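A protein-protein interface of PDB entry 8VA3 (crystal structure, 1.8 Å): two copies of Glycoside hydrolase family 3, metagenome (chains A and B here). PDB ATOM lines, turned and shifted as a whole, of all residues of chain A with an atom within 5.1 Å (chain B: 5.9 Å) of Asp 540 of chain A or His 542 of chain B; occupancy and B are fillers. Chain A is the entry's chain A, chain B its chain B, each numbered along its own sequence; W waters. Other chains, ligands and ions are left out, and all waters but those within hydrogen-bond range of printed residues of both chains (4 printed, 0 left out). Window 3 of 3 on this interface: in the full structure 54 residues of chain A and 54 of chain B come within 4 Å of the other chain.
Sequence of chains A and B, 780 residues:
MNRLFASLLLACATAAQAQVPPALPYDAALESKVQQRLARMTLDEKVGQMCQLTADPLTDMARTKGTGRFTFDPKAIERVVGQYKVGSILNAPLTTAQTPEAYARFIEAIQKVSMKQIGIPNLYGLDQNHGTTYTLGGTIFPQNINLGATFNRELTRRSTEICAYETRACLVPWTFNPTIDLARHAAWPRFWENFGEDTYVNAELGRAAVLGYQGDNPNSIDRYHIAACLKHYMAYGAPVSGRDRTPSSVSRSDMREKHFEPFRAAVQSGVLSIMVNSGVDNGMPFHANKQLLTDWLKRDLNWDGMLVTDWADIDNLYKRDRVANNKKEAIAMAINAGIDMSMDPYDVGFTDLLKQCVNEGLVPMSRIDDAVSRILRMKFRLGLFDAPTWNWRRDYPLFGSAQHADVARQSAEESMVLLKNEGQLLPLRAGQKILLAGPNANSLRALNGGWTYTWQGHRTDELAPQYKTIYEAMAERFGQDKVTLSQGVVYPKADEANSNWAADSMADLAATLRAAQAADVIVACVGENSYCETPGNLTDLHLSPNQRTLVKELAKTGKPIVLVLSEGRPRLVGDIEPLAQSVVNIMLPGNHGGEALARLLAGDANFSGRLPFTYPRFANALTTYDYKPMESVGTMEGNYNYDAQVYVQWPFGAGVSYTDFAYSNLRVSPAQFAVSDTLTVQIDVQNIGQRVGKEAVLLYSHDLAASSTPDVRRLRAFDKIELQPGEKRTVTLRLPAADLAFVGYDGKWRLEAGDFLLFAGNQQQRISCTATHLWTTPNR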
ATOM      1  N   LEU A 538     -21.112  16.900  14.294  1.00  0.00           N
ATOM      2  CA  LEU A 538     -20.028  17.492  13.516  1.00  0.00           C
ATOM      3  C   LEU A 538     -19.943  16.812  12.152  1.00  0.00           C
ATOM      4  O   LEU A 538     -20.517  15.742  11.929  1.00  0.00           O
ATOM      5  CB  LEU A 538     -18.676  17.415  14.267  1.00  0.00           C
ATOM      6  CG  LEU A 538     -18.019  16.087  14.670  1.00  0.00           C
ATOM      7  CD1 LEU A 538     -17.540  15.252  13.468  1.00  0.00           C
ATOM      8  CD2 LEU A 538     -16.845  16.321  15.611  1.00  0.00           C
ATOM      9  N   THR A 539     -19.225  17.442  11.225  1.00  0.00           N
ATOM     10  CA  THR A 539     -19.042  16.851   9.905  1.00  0.00           C
ATOM     11  C   THR A 539     -17.606  16.451   9.617  1.00  0.00           C
ATOM     12  O   THR A 539     -17.380  15.702   8.660  1.00  0.00           O
ATOM     13  CB  THR A 539     -19.503  17.823   8.798  1.00  0.00           C
ATOM     14  OG1 THR A 539     -18.850  19.083   8.985  1.00  0.00           O
ATOM     15  CG2 THR A 539     -21.008  18.045   8.878  1.00  0.00           C
ATOM     16  N   ASP A 540     -16.639  16.936  10.408  1.00  0.00           N
ATOM     17  CA  ASP A 540     -15.229  16.573  10.234  1.00  0.00           C
ATOM     18  C   ASP A 540     -14.577  16.586  11.605  1.00  0.00           C
ATOM     19  O   ASP A 540     -14.660  17.596  12.302  1.00  0.00           O
ATOM     20  CB  ASP A 540     -14.508  17.569   9.323  1.00  0.00           C
ATOM     21  CG  ASP A 540     -13.147  17.075   8.893  1.00  0.00           C
ATOM     22  OD1 ASP A 540     -12.255  16.979   9.752  1.00  0.00           O
ATOM     23  OD2 ASP A 540     -12.987  16.753   7.695  1.00  0.00           O
ATOM     24  N   LEU A 541     -13.909  15.491  11.977  1.00  0.00           N
ATOM     25  CA  LEU A 541     -13.315  15.400  13.316  1.00  0.00           C
ATOM     26  C   LEU A 541     -12.121  16.322  13.544  1.00  0.00           C
ATOM     27  O   LEU A 541     -11.706  16.473  14.701  1.00  0.00           O
ATOM     28  CB  LEU A 541     -12.869  13.956  13.591  1.00  0.00           C
ATOM     29  CG  LEU A 541     -13.923  13.070  14.227  1.00  0.00           C
ATOM     30  CD1 LEU A 541     -13.548  11.578  14.071  1.00  0.00           C
ATOM     31  CD2 LEU A 541     -14.092  13.455  15.738  1.00  0.00           C
ATOM     32  N   HIS A 542     -11.537  16.912  12.500  1.00  0.00           N
ATOM     33  CA  HIS A 542     -10.355  17.748  12.701  1.00  0.00           C
ATOM     34  C   HIS A 542     -10.634  18.883  13.686  1.00  0.00           C
ATOM     35  O   HIS A 542     -11.701  19.505  13.656  1.00  0.00           O
ATOM     36  CB  HIS A 542      -9.905  18.374  11.377  1.00  0.00           C
ATOM     37  CG  HIS A 542      -9.081  17.475  10.517  1.00  0.00           C
ATOM     38  ND1 HIS A 542      -9.616  16.711   9.503  1.00  0.00           N
ATOM     39  CD2 HIS A 542      -7.752  17.239  10.510  1.00  0.00           C
ATOM     40  CE1 HIS A 542      -8.646  16.034   8.910  1.00  0.00           C
ATOM     41  NE2 HIS A 542      -7.504  16.338   9.500  1.00  0.00           N
ATOM     42  N   ARG A 571     -10.816  15.475  19.029  1.00  0.00           N
ATOM     43  CA  ARG A 571     -10.643  16.116  17.735  1.00  0.00           C
ATOM     44  C   ARG A 571      -9.214  15.922  17.232  1.00  0.00           C
ATOM     45  O   ARG A 571      -8.258  15.904  18.015  1.00  0.00           O
ATOM     46  CB  ARG A 571     -10.989  17.610  17.833  1.00  0.00           C
ATOM     47  CG  ARG A 571     -12.398  17.864  18.491  1.00  0.00           C
ATOM     48  CD  ARG A 571     -13.542  17.318  17.614  1.00  0.00           C
ATOM     49  NE  ARG A 571     -13.594  18.025  16.336  1.00  0.00           N
ATOM     50  CZ  ARG A 571     -14.335  19.099  16.089  1.00  0.00           C
ATOM     51  NH1 ARG A 571     -15.213  19.557  16.978  1.00  0.00           N
ATOM     52  NH2 ARG A 571     -14.214  19.715  14.911  1.00  0.00           N
ATOM     53  N   ALA A 619      -9.451  11.059   9.957  1.00  0.00           N
ATOM     54  CA  ALA A 619     -10.906  11.156   9.947  1.00  0.00           C
ATOM     55  C   ALA A 619     -11.566   9.904   9.390  1.00  0.00           C
ATOM     56  O   ALA A 619     -12.697   9.572   9.770  1.00  0.00           O
ATOM     57  CB  ALA A 619     -11.325  12.395   9.147  1.00  0.00           C
ATOM     58  N   ASP B 540      -8.109   9.555   4.700  1.00  0.00           N
ATOM     59  CA  ASP B 540      -8.928  10.748   4.673  1.00  0.00           C
ATOM     60  C   ASP B 540      -9.498  10.872   3.269  1.00  0.00           C
ATOM     61  O   ASP B 540      -8.760  10.821   2.288  1.00  0.00           O
ATOM     62  CB  ASP B 540      -8.104  11.970   5.090  1.00  0.00           C
ATOM     63  CG  ASP B 540      -8.984  13.224   5.272  1.00  0.00           C
ATOM     64  OD1 ASP B 540      -9.679  13.574   4.317  1.00  0.00           O
ATOM     65  OD2 ASP B 540      -9.011  13.826   6.374  1.00  0.00           O
ATOM     66  N   LEU B 541     -10.811  10.986   3.175  1.00  0.00           N
ATOM     67  CA  LEU B 541     -11.459  11.023   1.858  1.00  0.00           C
ATOM     68  C   LEU B 541     -11.159  12.288   1.043  1.00  0.00           C
ATOM     69  O   LEU B 541     -11.460  12.299  -0.150  1.00  0.00           O
ATOM     70  CB  LEU B 541     -12.978  10.907   2.041  1.00  0.00           C
ATOM     71  CG  LEU B 541     -13.479   9.459   2.056  1.00  0.00           C
ATOM     72  CD1 LEU B 541     -14.860   9.377   2.726  1.00  0.00           C
ATOM     73  CD2 LEU B 541     -13.515   8.929   0.612  1.00  0.00           C
ATOM     74  N   HIS B 542     -10.672  13.378   1.650  1.00  0.00           N
ATOM     75  CA  HIS B 542     -10.438  14.597   0.865  1.00  0.00           C
ATOM     76  C   HIS B 542      -9.578  14.325  -0.370  1.00  0.00           C
ATOM     77  O   HIS B 542      -8.583  13.595  -0.300  1.00  0.00           O
ATOM     78  CB  HIS B 542      -9.737  15.670   1.715  1.00  0.00           C
ATOM     79  CG  HIS B 542     -10.667  16.439   2.627  1.00  0.00           C
ATOM     80  ND1 HIS B 542     -10.969  16.013   3.901  1.00  0.00           N
ATOM     81  CD2 HIS B 542     -11.395  17.567   2.426  1.00  0.00           C
ATOM     82  CE1 HIS B 542     -11.817  16.861   4.461  1.00  0.00           C
ATOM     83  NE2 HIS B 542     -12.104  17.804   3.583  1.00  0.00           N
ATOM     84  N   LEU B 543      -9.915  14.987  -1.491  1.00  0.00           N
ATOM     85  CA  LEU B 543      -8.962  15.110  -2.594  1.00  0.00           C
ATOM     86  C   LEU B 543      -7.611  15.603  -2.076  1.00  0.00           C
ATOM     87  O   LEU B 543      -7.533  16.365  -1.107  1.00  0.00           O
ATOM     88  CB  LEU B 543      -9.499  16.085  -3.660  1.00  0.00           C
ATOM     89  CG  LEU B 543      -8.661  16.221  -4.922  1.00  0.00           C
ATOM     90  CD1 LEU B 543      -8.790  14.934  -5.724  1.00  0.00           C
ATOM     91  CD2 LEU B 543      -9.146  17.444  -5.725  1.00  0.00           C
ATOM     92  N   SER B 544      -6.529  15.171  -2.728  1.00  0.00           N
ATOM     93  CA  SER B 544      -5.204  15.515  -2.227  1.00  0.00           C
ATOM     94  C   SER B 544      -4.996  17.029  -2.158  1.00  0.00           C
ATOM     95  O   SER B 544      -5.537  17.799  -2.978  1.00  0.00           O
ATOM     96  CB  SER B 544      -4.114  14.898  -3.106  1.00  0.00           C
ATOM     97  OG  SER B 544      -3.851  15.730  -4.230  1.00  0.00           O
ATOM     98  N   ARG B 548      -6.273  20.108  -4.741  1.00  0.00           N
ATOM     99  CA  ARG B 548      -7.134  21.208  -4.312  1.00  0.00           C
ATOM    100  C   ARG B 548      -6.479  22.555  -4.627  1.00  0.00           C
ATOM    101  O   ARG B 548      -7.111  23.461  -5.194  1.00  0.00           O
ATOM    102  CB  ARG B 548      -7.433  21.070  -2.816  1.00  0.00           C
ATOM    103  CG  ARG B 548      -8.245  19.810  -2.438  1.00  0.00           C
ATOM    104  CD  ARG B 548      -8.195  19.560  -0.931  1.00  0.00           C
ATOM    105  NE  ARG B 548      -8.950  20.499  -0.108  1.00  0.00           N
ATOM    106  CZ  ARG B 548      -9.047  20.408   1.219  1.00  0.00           C
ATOM    107  NH1 ARG B 548      -8.449  19.436   1.893  1.00  0.00           N
ATOM    108  NH2 ARG B 548      -9.765  21.308   1.887  1.00  0.00           N
ATOM    109  N   ARG B 571     -13.782  11.174  -3.927  1.00  0.00           N
ATOM    110  CA  ARG B 571     -12.969  12.011  -3.058  1.00  0.00           C
ATOM    111  C   ARG B 571     -13.598  13.397  -2.872  1.00  0.00           C
ATOM    112  O   ARG B 571     -14.213  13.955  -3.784  1.00  0.00           O
ATOM    113  CB  ARG B 571     -11.568  12.139  -3.658  1.00  0.00           C
ATOM    114  CG  ARG B 571     -10.921  10.745  -3.915  1.00  0.00           C
ATOM    115  CD  ARG B 571     -10.738   9.900  -2.631  1.00  0.00           C
ATOM    116  NE  ARG B 571      -9.755  10.498  -1.742  1.00  0.00           N
ATOM    117  CZ  ARG B 571      -8.443  10.264  -1.791  1.00  0.00           C
ATOM    118  NH1 ARG B 571      -7.925   9.324  -2.575  1.00  0.00           N
ATOM    119  NH2 ARG B 571      -7.625  10.996  -1.035  1.00  0.00           N
ATOM    120  N   LEU B 572     -13.403  13.975  -1.688  1.00  0.00           N
ATOM    121  CA  LEU B 572     -14.168  15.169  -1.336  1.00  0.00           C
ATOM    122  C   LEU B 572     -13.646  16.374  -2.120  1.00  0.00           C
ATOM    123  O   LEU B 572     -12.440  16.625  -2.148  1.00  0.00           O
ATOM    124  CB  LEU B 572     -14.095  15.468   0.165  1.00  0.00           C
ATOM    125  CG  LEU B 572     -14.353  14.271   1.090  1.00  0.00           C
ATOM    126  CD1 LEU B 572     -14.257  14.709   2.535  1.00  0.00           C
ATOM    127  CD2 LEU B 572     -15.701  13.651   0.778  1.00  0.00           C
ATOM    128  N   ASP B 575     -14.718  22.084  -1.477  1.00  0.00           N
ATOM    129  CA  ASP B 575     -14.078  23.398  -1.522  1.00  0.00           C
ATOM    130  C   ASP B 575     -13.696  23.848  -2.938  1.00  0.00           C
ATOM    131  O   ASP B 575     -13.355  25.017  -3.122  1.00  0.00           O
ATOM    132  CB  ASP B 575     -12.826  23.417  -0.631  1.00  0.00           C
ATOM    133  CG  ASP B 575     -11.785  22.391  -1.073  1.00  0.00           C
ATOM    134  OD1 ASP B 575     -12.188  21.395  -1.689  1.00  0.00           O
ATOM    135  OD2 ASP B 575     -10.590  22.545  -0.776  1.00  0.00           O
ATOM    136  N   ARG B 617     -20.040  14.975   0.926  1.00  0.00           N
ATOM    137  CA  ARG B 617     -19.450  16.285   1.098  1.00  0.00           C
ATOM    138  C   ARG B 617     -18.373  16.299   2.172  1.00  0.00           C
ATOM    139  O   ARG B 617     -17.388  17.010   2.029  1.00  0.00           O
ATOM    140  CB  ARG B 617     -20.572  17.277   1.486  1.00  0.00           C
ATOM    141  CG  ARG B 617     -20.339  18.704   1.241  1.00  0.00           C
ATOM    142  CD  ARG B 617     -21.606  19.508   1.628  1.00  0.00           C
ATOM    143  NE  ARG B 617     -22.696  19.428   0.652  1.00  0.00           N
ATOM    144  CZ  ARG B 617     -22.805  20.223  -0.412  1.00  0.00           C
ATOM    145  NH1 ARG B 617     -21.828  21.037  -0.769  1.00  0.00           N
ATOM    146  NH2 ARG B 617     -23.931  20.221  -1.115  1.00  0.00           N
ATOM    147  N   PHE B 618     -18.570  15.563   3.270  1.00  0.00           N
ATOM    148  CA  PHE B 618     -17.743  15.677   4.462  1.00  0.00           C
ATOM    149  C   PHE B 618     -17.250  14.300   4.914  1.00  0.00           C
ATOM    150  O   PHE B 618     -17.978  13.303   4.859  1.00  0.00           O
ATOM    151  CB  PHE B 618     -18.520  16.287   5.634  1.00  0.00           C
ATOM    152  CG  PHE B 618     -19.142  17.642   5.340  1.00  0.00           C
ATOM    153  CD1 PHE B 618     -18.342  18.761   5.180  1.00  0.00           C
ATOM    154  CD2 PHE B 618     -20.538  17.794   5.322  1.00  0.00           C
ATOM    155  CE1 PHE B 618     -18.908  20.023   4.948  1.00  0.00           C
ATOM    156  CE2 PHE B 618     -21.121  19.052   5.093  1.00  0.00           C
ATOM    157  CZ  PHE B 618     -20.308  20.160   4.896  1.00  0.00           C
ATOM    158  N   ALA B 619     -16.031  14.285   5.451  1.00  0.00           N
ATOM    159  CA  ALA B 619     -15.383  13.029   5.823  1.00  0.00           C
ATOM    160  C   ALA B 619     -16.136  12.284   6.927  1.00  0.00           C
ATOM    161  O   ALA B 619     -16.125  11.056   6.952  1.00  0.00           O
ATOM    162  CB  ALA B 619     -13.952  13.312   6.274  1.00  0.00           C
ATOM    163  N   ASN B 620     -16.792  12.989   7.861  1.00  0.00           N
ATOM    164  CA  ASN B 620     -17.470  12.288   8.946  1.00  0.00           C
ATOM    165  C   ASN B 620     -18.994  12.467   8.895  1.00  0.00           C
ATOM    166  O   ASN B 620     -19.668  12.431   9.925  1.00  0.00           O
ATOM    167  CB  ASN B 620     -16.886  12.723  10.289  1.00  0.00           C
ATOM    168  CG  ASN B 620     -15.441  12.256  10.469  1.00  0.00           C
ATOM    169  OD1 ASN B 620     -14.533  13.080  10.490  1.00  0.00           O
ATOM    170  ND2 ASN B 620     -15.220  10.920  10.587  1.00  0.00           N
ATOM    171  N   ALA B 621     -19.553  12.643   7.698  1.00  0.00           N
ATOM    172  CA  ALA B 621     -21.001  12.626   7.526  1.00  0.00           C
ATOM    173  C   ALA B 621     -21.302  11.817   6.271  1.00  0.00           C
ATOM    174  O   ALA B 621     -21.803  12.297   5.270  1.00  0.00           O
ATOM    175  CB  ALA B 621     -21.591  14.039   7.460  1.00  0.00           C
HETATM  176  O   HOH W   1     -10.607  15.819   6.927  1.00  0.00           O
HETATM  177  O   HOH W   2     -20.890  12.361  12.456  1.00  0.00           O
HETATM  178  O   HOH W   3     -14.757  16.843   5.788  1.00  0.00           O
HETATM  179  O   HOH W   4      -7.819  12.846   8.521  1.00  0.00           O
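The backbone carbonyl oxygen of Thr 539 of chain A sits at hydrogen-bond distance from the backbone NH of Asn 620 of chain B, 2.9 Å away.
The backbone NH (N) of Leu 541 of chain A is in hydrogen-bond range of the side-chain amide oxygen (OD1) of Asn 620 of chain B (2.9 Å).
The side-chain amide nitrogen (ND2) of Asn 620 of chain B sits at hydrogen-bond distance from the backbone carbonyl oxygen (O) of Ala 619 of chain A, at 3.0 Å.
The side-chain carboxylate (OD1) of Asp 540 of chain A sits at hydrogen-bond distance from a ring nitrogen (ND1) of His 542 of chain A (2.7 Å).
The backbone carbonyl oxygen (O) of Asp 540 of chain A lies within hydrogen-bond range of the guanidinium group (NH2) of Arg 571 of chain A.
O of Leu 541 of chain A lies within hydrogen-bond range of NE of Arg 571 of chain A.
The backbone carbonyl oxygen (O) of His 542 of chain A is in hydrogen-bond range of the guanidinium group (NH2) of Arg 571 of chain A (2.8 Å).
The side-chain carboxylate of Asp 540 of chain B is in hydrogen-bond range of a ring nitrogen (ND1) of His 542 of chain B, 2.8 Å away.
The backbone carbonyl oxygen of His 542 of chain B sits at hydrogen-bond distance from the guanidinium group of Arg 571 of chain B (2.9 Å).
Among the printed residues, pairs that only touch across the chains: Leu 538 of chain A with Asn 620 of chain B, Thr 539 of chain A with Phe 618 of chain B, Thr 539 of chain A with Ala 619 of chain B, Thr 539 of chain A with Ala 621 of chain B, Asp 540 of chain A with His 542 of chain B, Asp 540 of chain A with Ala 619 of chain B, Asp 540 of chain A with Asn 620 of chain B, His 542 of chain A with Asp 540 of chain B, Ala 619 of chain A with Asp 540 of chain B and Ala 619 of chain A with Ala 619 of chain B.
Of chain B, only His 542, Ala 619 and Asn 620 come within 4 Å of Asp 540 of chain A.
Of chain A, only Asp 540 comes within 4 Å of His 542 of chain B.
Of the printed residues of chain A, Ala 619 of chain B touches Thr 539 (3.8 Å), Asp 540 (3.8 Å) and Ala 619 (3.9995 Å).
Of the printed residues of chain B, Ala 619 of chain A touches Asp 540, Ala 619 and Asn 620.
Of the printed residues of chain B, His 542 of chain A touches Asp 540 (3.4 Å).
Of the printed residues of chain A, Ala 621 of chain B touches Thr 539.
Arg 548 of chain B touches none of the printed residues of chain A.
The nearest residue of chain B that does not touch Asp 540 of chain A is Asp 540 of chain B (5.1 Å).
The nearest printed residue of chain A that does not touch His 542 of chain B is His 542 of chain A (5.5 Å).
The nearest printed residue of chain A that does not touch Phe 618 of chain B is Asp 540 of chain A (5.2 Å).
Of the 7 printed residues of chain A, 6 touch a printed residue of chain B.
Printed residues of chain A that touch a printed residue of chain B: Leu 538, Thr 539, Asp 540, Leu 541, His 542 and Ala 619.
Hydrophobic or aromatic side chains of chain A within 4 Å of the printed part of chain B: Leu 541, His 542 and Ala 619.
Among the printed residues, 13 pairs touch across the chains.
Among the printed residues, no Asp or Glu carboxylate lies within 4 Å of a Lys or Arg side-chain nitrogen of the other chain.
Asp 540 of chain A touches His 542 of chain B, and with the chains exchanged His 542 of chain A touches Asp 540 of chain B.
Asp 540 of chain A touches Ala 619 of chain B, and with the chains exchanged Ala 619 of chain A touches Asp 540 of chain B.
Ala 619 of chain B touches its own counterpart, Ala 619 of chain A.
5 positions are printed for both chains.
Of the 13 pairs that touch across the chains among the printed residues, 5 have their exchanged pair printed and touching as well.
Water W3 lies within hydrogen-bond range of OD2 of Asp 540 of chain A (2.6 Å) and N of Ala 619 of chain B (2.9 Å).
Water W1 lies within hydrogen-bond range of OD2 of Asp 540 of chain B (2.6 Å), OD2 of Asp 540 of chain A (2.7 Å), ND1 of His 542 of chain A (2.9 Å) and ND1 of His 542 of chain B (3.1 Å).
Water W4 bridges OD2 of Asp 540 of chain B and N of Ala 619 of chain A.
Water W2 bridges O of Asn 620 of chain B (2.8 Å) and O of Leu 538 of chain A (3.4 Å).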
